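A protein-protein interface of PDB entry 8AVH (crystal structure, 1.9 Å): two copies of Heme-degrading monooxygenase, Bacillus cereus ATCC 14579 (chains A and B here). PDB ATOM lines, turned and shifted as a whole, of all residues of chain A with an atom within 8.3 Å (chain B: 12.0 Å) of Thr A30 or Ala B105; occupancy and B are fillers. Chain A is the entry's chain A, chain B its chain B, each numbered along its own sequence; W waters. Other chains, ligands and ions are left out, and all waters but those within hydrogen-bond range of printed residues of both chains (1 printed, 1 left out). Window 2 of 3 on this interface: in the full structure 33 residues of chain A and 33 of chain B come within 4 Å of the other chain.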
ATOM      1  N   VAL A  25     -30.467  33.644  -8.282  1.00  0.00           N
ATOM      2  CA  VAL A  25     -29.272  32.987  -7.759  1.00  0.00           C
ATOM      3  C   VAL A  25     -28.928  33.608  -6.411  1.00  0.00           C
ATOM      4  O   VAL A  25     -29.003  34.825  -6.247  1.00  0.00           O
ATOM      5  CB  VAL A  25     -28.107  33.109  -8.758  1.00  0.00           C
ATOM      6  CG1 VAL A  25     -26.818  32.622  -8.134  1.00  0.00           C
ATOM      7  CG2 VAL A  25     -28.401  32.317 -10.043  1.00  0.00           C
ATOM      8  N   GLY A  26     -28.569  32.775  -5.431  1.00  0.00           N
ATOM      9  CA  GLY A  26     -28.304  33.276  -4.098  1.00  0.00           C
ATOM     10  C   GLY A  26     -27.014  32.738  -3.518  1.00  0.00           C
ATOM     11  O   GLY A  26     -26.129  32.279  -4.245  1.00  0.00           O
ATOM     12  N   LYS A  27     -26.897  32.783  -2.200  1.00  0.00           N
ATOM     13  CA  LYS A  27     -25.680  32.341  -1.537  1.00  0.00           C
ATOM     14  C   LYS A  27     -25.750  30.912  -1.015  1.00  0.00           C
ATOM     15  O   LYS A  27     -24.701  30.269  -0.881  1.00  0.00           O
ATOM     16  CB  LYS A  27     -25.352  33.285  -0.376  1.00  0.00           C
ATOM     17  CG  LYS A  27     -24.852  34.648  -0.843  1.00  0.00           C
ATOM     18  CD  LYS A  27     -23.787  34.464  -1.922  1.00  0.00           C
ATOM     19  CE  LYS A  27     -23.152  35.788  -2.342  1.00  0.00           C
ATOM     20  NZ  LYS A  27     -22.356  36.396  -1.234  1.00  0.00           N
ATOM     21  N   VAL A  28     -26.948  30.402  -0.716  1.00  0.00           N
ATOM     22  CA  VAL A  28     -27.041  29.086  -0.094  1.00  0.00           C
ATOM     23  C   VAL A  28     -26.449  28.025  -1.011  1.00  0.00           C
ATOM     24  O   VAL A  28     -25.871  27.043  -0.533  1.00  0.00           O
ATOM     25  CB  VAL A  28     -28.495  28.757   0.314  1.00  0.00           C
ATOM     26  CG1 VAL A  28     -29.406  28.588  -0.917  1.00  0.00           C
ATOM     27  CG2 VAL A  28     -28.532  27.487   1.177  1.00  0.00           C
ATOM     28  N   GLU A  29     -26.519  28.228  -2.336  1.00  0.00           N
ATOM     29  CA  GLU A  29     -25.977  27.236  -3.251  1.00  0.00           C
ATOM     30  C   GLU A  29     -24.450  27.213  -3.281  1.00  0.00           C
ATOM     31  O   GLU A  29     -23.885  26.319  -3.924  1.00  0.00           O
ATOM     32  CB  GLU A  29     -26.531  27.440  -4.673  1.00  0.00           C
ATOM     33  CG  GLU A  29     -26.508  28.862  -5.224  1.00  0.00           C
ATOM     34  CD  GLU A  29     -27.856  29.572  -5.063  1.00  0.00           C
ATOM     35  OE1 GLU A  29     -28.266  29.827  -3.912  1.00  0.00           O
ATOM     36  OE2 GLU A  29     -28.516  29.875  -6.096  1.00  0.00           O
ATOM     37  N   THR A  30     -23.774  28.148  -2.609  1.00  0.00           N
ATOM     38  CA  THR A  30     -22.320  28.110  -2.474  1.00  0.00           C
ATOM     39  C   THR A  30     -21.857  27.398  -1.204  1.00  0.00           C
ATOM     40  O   THR A  30     -20.651  27.344  -0.950  1.00  0.00           O
ATOM     41  CB  THR A  30     -21.733  29.533  -2.471  1.00  0.00           C
ATOM     42  OG1 THR A  30     -22.226  30.254  -1.333  1.00  0.00           O
ATOM     43  CG2 THR A  30     -22.124  30.279  -3.733  1.00  0.00           C
ATOM     44  N   MET A  31     -22.772  26.872  -0.396  1.00  0.00           N
ATOM     45  CA  MET A  31     -22.410  26.324   0.903  1.00  0.00           C
ATOM     46  C   MET A  31     -21.885  24.893   0.777  1.00  0.00           C
ATOM     47  O   MET A  31     -22.351  24.123  -0.063  1.00  0.00           O
ATOM     48  CB  MET A  31     -23.609  26.344   1.839  1.00  0.00           C
ATOM     49  CG  MET A  31     -24.083  27.721   2.222  1.00  0.00           C
ATOM     50  SD  MET A  31     -22.864  28.619   3.234  1.00  0.00           S
ATOM     51  CE  MET A  31     -22.471  30.012   2.184  1.00  0.00           C
ATOM     52  N   PRO A  32     -20.910  24.520   1.602  1.00  0.00           N
ATOM     53  CA  PRO A  32     -20.428  23.129   1.607  1.00  0.00           C
ATOM     54  C   PRO A  32     -21.552  22.152   1.915  1.00  0.00           C
ATOM     55  O   PRO A  32     -22.374  22.388   2.799  1.00  0.00           O
ATOM     56  CB  PRO A  32     -19.367  23.120   2.720  1.00  0.00           C
ATOM     57  CG  PRO A  32     -18.913  24.559   2.818  1.00  0.00           C
ATOM     58  CD  PRO A  32     -20.132  25.397   2.493  1.00  0.00           C
ATOM     59  N   GLY A  33     -21.576  21.039   1.179  1.00  0.00           N
ATOM     60  CA  GLY A  33     -22.586  20.012   1.395  1.00  0.00           C
ATOM     61  C   GLY A  33     -23.961  20.320   0.830  1.00  0.00           C
ATOM     62  O   GLY A  33     -24.858  19.475   0.933  1.00  0.00           O
ATOM     63  N   PHE A  34     -24.156  21.493   0.227  1.00  0.00           N
ATOM     64  CA  PHE A  34     -25.431  21.806  -0.419  1.00  0.00           C
ATOM     65  C   PHE A  34     -25.592  20.977  -1.676  1.00  0.00           C
ATOM     66  O   PHE A  34     -24.662  20.853  -2.482  1.00  0.00           O
ATOM     67  CB  PHE A  34     -25.488  23.298  -0.733  1.00  0.00           C
ATOM     68  CG  PHE A  34     -26.695  23.734  -1.548  1.00  0.00           C
ATOM     69  CD1 PHE A  34     -26.630  23.798  -2.926  1.00  0.00           C
ATOM     70  CD2 PHE A  34     -27.870  24.122  -0.914  1.00  0.00           C
ATOM     71  CE1 PHE A  34     -27.730  24.242  -3.683  1.00  0.00           C
ATOM     72  CE2 PHE A  34     -28.971  24.563  -1.645  1.00  0.00           C
ATOM     73  CZ  PHE A  34     -28.889  24.637  -3.041  1.00  0.00           C
ATOM     74  N   TRP A  57     -29.125  18.322   1.491  1.00  0.00           N
ATOM     75  CA  TRP A  57     -27.796  18.471   2.075  1.00  0.00           C
ATOM     76  C   TRP A  57     -27.172  17.094   2.274  1.00  0.00           C
ATOM     77  O   TRP A  57     -27.868  16.114   2.531  1.00  0.00           O
ATOM     78  CB  TRP A  57     -27.852  19.203   3.428  1.00  0.00           C
ATOM     79  CG  TRP A  57     -28.504  20.542   3.342  1.00  0.00           C
ATOM     80  CD1 TRP A  57     -29.840  20.799   3.358  1.00  0.00           C
ATOM     81  CD2 TRP A  57     -27.853  21.796   3.159  1.00  0.00           C
ATOM     82  NE1 TRP A  57     -30.063  22.144   3.235  1.00  0.00           N
ATOM     83  CE2 TRP A  57     -28.862  22.783   3.103  1.00  0.00           C
ATOM     84  CE3 TRP A  57     -26.510  22.188   3.069  1.00  0.00           C
ATOM     85  CZ2 TRP A  57     -28.577  24.141   2.956  1.00  0.00           C
ATOM     86  CZ3 TRP A  57     -26.226  23.548   2.918  1.00  0.00           C
ATOM     87  CH2 TRP A  57     -27.260  24.503   2.856  1.00  0.00           C
ATOM     88  N   TRP A  66     -24.892  26.479   7.343  1.00  0.00           N
ATOM     89  CA  TRP A  66     -25.470  27.597   6.603  1.00  0.00           C
ATOM     90  C   TRP A  66     -26.281  28.497   7.525  1.00  0.00           C
ATOM     91  O   TRP A  66     -26.147  29.722   7.470  1.00  0.00           O
ATOM     92  CB  TRP A  66     -26.327  27.106   5.432  1.00  0.00           C
ATOM     93  CG  TRP A  66     -27.070  28.248   4.754  1.00  0.00           C
ATOM     94  CD1 TRP A  66     -26.519  29.394   4.213  1.00  0.00           C
ATOM     95  CD2 TRP A  66     -28.480  28.363   4.571  1.00  0.00           C
ATOM     96  NE1 TRP A  66     -27.509  30.197   3.702  1.00  0.00           N
ATOM     97  CE2 TRP A  66     -28.722  29.593   3.915  1.00  0.00           C
ATOM     98  CE3 TRP A  66     -29.566  27.551   4.899  1.00  0.00           C
ATOM     99  CZ2 TRP A  66     -30.004  30.019   3.573  1.00  0.00           C
ATOM    100  CZ3 TRP A  66     -30.847  27.978   4.554  1.00  0.00           C
ATOM    101  CH2 TRP A  66     -31.054  29.200   3.901  1.00  0.00           C
ATOM    102  N   SER A  69     -24.325  30.958   9.176  1.00  0.00           N
ATOM    103  CA  SER A  69     -23.382  31.657   8.318  1.00  0.00           C
ATOM    104  C   SER A  69     -23.672  33.154   8.246  1.00  0.00           C
ATOM    105  O   SER A  69     -24.756  33.638   8.592  1.00  0.00           O
ATOM    106  CB  SER A  69     -23.416  31.087   6.904  1.00  0.00           C
ATOM    107  OG  SER A  69     -24.634  31.450   6.272  1.00  0.00           O
ATOM    108  N   ALA A  71     -23.753  34.777   5.240  1.00  0.00           N
ATOM    109  CA  ALA A  71     -24.671  34.942   4.118  1.00  0.00           C
ATOM    110  C   ALA A  71     -26.113  34.656   4.517  1.00  0.00           C
ATOM    111  O   ALA A  71     -27.037  35.270   3.975  1.00  0.00           O
ATOM    112  CB  ALA A  71     -24.246  34.039   2.961  1.00  0.00           C
ATOM    113  N   VAL B  99     -35.473  25.742  -9.582  1.00  0.00           N
ATOM    114  CA  VAL B  99     -34.424  24.786  -9.228  1.00  0.00           C
ATOM    115  C   VAL B  99     -33.097  25.518  -9.172  1.00  0.00           C
ATOM    116  O   VAL B  99     -32.632  26.043 -10.192  1.00  0.00           O
ATOM    117  CB  VAL B  99     -34.334  23.624 -10.225  1.00  0.00           C
ATOM    118  CG1 VAL B  99     -33.156  22.724  -9.835  1.00  0.00           C
ATOM    119  CG2 VAL B  99     -35.643  22.859 -10.260  1.00  0.00           C
ATOM    120  N   ARG B 100     -32.474  25.539  -8.001  1.00  0.00           N
ATOM    121  CA  ARG B 100     -31.166  26.170  -7.825  1.00  0.00           C
ATOM    122  C   ARG B 100     -30.141  25.107  -7.446  1.00  0.00           C
ATOM    123  O   ARG B 100     -30.192  24.555  -6.341  1.00  0.00           O
ATOM    124  CB  ARG B 100     -31.242  27.271  -6.777  1.00  0.00           C
ATOM    125  CG  ARG B 100     -31.838  28.561  -7.363  1.00  0.00           C
ATOM    126  CD  ARG B 100     -32.492  29.429  -6.299  1.00  0.00           C
ATOM    127  NE  ARG B 100     -31.515  29.955  -5.353  1.00  0.00           N
ATOM    128  CZ  ARG B 100     -31.826  30.704  -4.298  1.00  0.00           C
ATOM    129  NH1 ARG B 100     -33.064  31.121  -4.080  1.00  0.00           N
ATOM    130  NH2 ARG B 100     -30.871  31.047  -3.441  1.00  0.00           N
ATOM    131  N   MET B 101     -29.231  24.807  -8.370  1.00  0.00           N
ATOM    132  CA  MET B 101     -28.202  23.785  -8.234  1.00  0.00           C
ATOM    133  C   MET B 101     -26.976  24.367  -7.536  1.00  0.00           C
ATOM    134  O   MET B 101     -26.841  25.596  -7.421  1.00  0.00           O
ATOM    135  CB  MET B 101     -27.813  23.238  -9.612  1.00  0.00           C
ATOM    136  CG  MET B 101     -28.932  22.524 -10.363  1.00  0.00           C
ATOM    137  SD  MET B 101     -29.624  21.154  -9.404  1.00  0.00           S
ATOM    138  CE  MET B 101     -28.197  20.057  -9.280  1.00  0.00           C
ATOM    139  N   PRO B 102     -26.087  23.516  -7.008  1.00  0.00           N
ATOM    140  CA  PRO B 102     -24.870  24.031  -6.365  1.00  0.00           C
ATOM    141  C   PRO B 102     -24.057  24.872  -7.341  1.00  0.00           C
ATOM    142  O   PRO B 102     -24.028  24.605  -8.546  1.00  0.00           O
ATOM    143  CB  PRO B 102     -24.115  22.758  -5.963  1.00  0.00           C
ATOM    144  CG  PRO B 102     -25.161  21.703  -5.882  1.00  0.00           C
ATOM    145  CD  PRO B 102     -26.128  22.040  -6.968  1.00  0.00           C
ATOM    146  N   MET B 103     -23.426  25.921  -6.809  1.00  0.00           N
ATOM    147  CA  MET B 103     -22.530  26.786  -7.565  1.00  0.00           C
ATOM    148  C   MET B 103     -21.229  26.948  -6.797  1.00  0.00           C
ATOM    149  O   MET B 103     -21.219  26.945  -5.562  1.00  0.00           O
ATOM    150  CB  MET B 103     -23.091  28.204  -7.793  1.00  0.00           C
ATOM    151  CG  MET B 103     -24.343  28.321  -8.614  1.00  0.00           C
ATOM    152  SD  MET B 103     -24.527  30.035  -9.167  1.00  0.00           S
ATOM    153  CE  MET B 103     -23.681  30.945  -7.856  1.00  0.00           C
ATOM    154  N   ALA B 104     -20.135  27.121  -7.530  1.00  0.00           N
ATOM    155  CA  ALA B 104     -18.873  27.463  -6.889  1.00  0.00           C
ATOM    156  C   ALA B 104     -18.971  28.850  -6.263  1.00  0.00           C
ATOM    157  O   ALA B 104     -19.555  29.769  -6.846  1.00  0.00           O
ATOM    158  CB  ALA B 104     -17.732  27.414  -7.901  1.00  0.00           C
ATOM    159  N   ALA B 105     -18.410  28.999  -5.057  1.00  0.00           N
ATOM    160  CA  ALA B 105     -18.454  30.289  -4.373  1.00  0.00           C
ATOM    161  C   ALA B 105     -17.573  31.345  -5.032  1.00  0.00           C
ATOM    162  O   ALA B 105     -17.638  32.514  -4.636  1.00  0.00           O
ATOM    163  CB  ALA B 105     -18.052  30.132  -2.906  1.00  0.00           C
ATOM    164  N   ALA B 106     -16.758  30.966  -6.014  1.00  0.00           N
ATOM    165  CA  ALA B 106     -15.966  31.923  -6.781  1.00  0.00           C
ATOM    166  C   ALA B 106     -16.772  32.440  -7.966  1.00  0.00           C
ATOM    167  O   ALA B 106     -17.203  31.663  -8.820  1.00  0.00           O
ATOM    168  CB  ALA B 106     -14.663  31.284  -7.259  1.00  0.00           C
HETATM  169  O   HOH W   1     -28.232  28.268  -8.144  1.00  0.00           O
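OE1 of Glu A29 is in salt-bridge range of NH2 of Arg B100 (2.9 Å). The backbone NH (N) of Met B103 is in hydrogen-bond range of the backbone carbonyl oxygen (O) of Glu A29. N of Gly A26 lies close to NH2 of Arg B100, at 3.5 Å.
The side-chain carboxylate (OE2) of Glu A29 lies within hydrogen-bond range of the backbone NH (N) of Gly A26. The backbone carbonyl oxygen (O) of Lys A27 sits at hydrogen-bond distance from the side-chain hydroxyl (OG1) of Thr A30 (2.5 Å).
Among the printed residues, merely in contact across the chains: Val A25 with Met B103 (3.6 Å), Val A28 with Arg B100 (3.8 Å), Glu A29 with Met B101 (3.3 Å), Glu A29 with Pro B102 (3.5 Å), Thr A30 with Met B103 (3.5 Å), Thr A30 with Ala B105 (3.7 Å), Phe A34 with Arg B100 (3.5 Å), Phe A34 with Met B101 (3.9 Å) and Phe A34 with Pro B102 (3.5 Å).
Of the printed residues of chain B, Val A25 touches Met B103 (3.6 Å). Gly A26 touches one residue of chain B. Lys A27 touches none of the printed residues of chain B. Val A28 touches just one residue of chain B: Arg B100. Printed residues of chain B within 4 Å of Glu A29: Arg B100, Met B101, Pro B102 and Met B103. Printed residues of chain B within 4 Å of Thr A30: Met B103 (3.5 Å) and Ala B105 (3.7 Å). No residue of chain B comes within 4 Å of Met A31. No residue of chain B comes within 4 Å of Pro A32. Phe A34 touches just these residues of chain B: Arg B100 (3.5 Å), Met B101 (3.9 Å) and Pro B102 (3.5 Å). Ala A71 touches none of the printed residues of chain B. Val B99 touches none of the printed residues of chain A. Printed residues of chain A within 4 Å of Pro B102: Glu A29 and Phe A34. Ala B105 touches just one residue of chain A: Thr A30. Ala B106 touches none of the printed residues of chain A. The nearest residue of chain A that does not touch Ala B105 is Glu A29 (6.2 Å). The nearest printed residue of chain B that does not touch Val A25 is Arg B100 (4.4 Å).
Of the 14 printed residues of chain A, 6 touch a printed residue of chain B. Of the 8 printed residues of chain B, 5 touch a printed residue of chain A. Hydrophobic or aromatic side chains of chain B that line the printed part of chain A: Pro B102, Met B103 and Ala B105. Among the printed residues, Asp or Glu carboxylates within 4 Å of a Lys or Arg side-chain nitrogen of the other chain: Glu A29 with Arg B100.
No position is printed for both chains. Of the 12 pairs that touch across the chains among the printed residues, none has its exchanged pair printed and touching as well.
Water W1 bridges OE2 of Glu A29 (2.6 Å) and O of Met B101 (3.1 Å).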
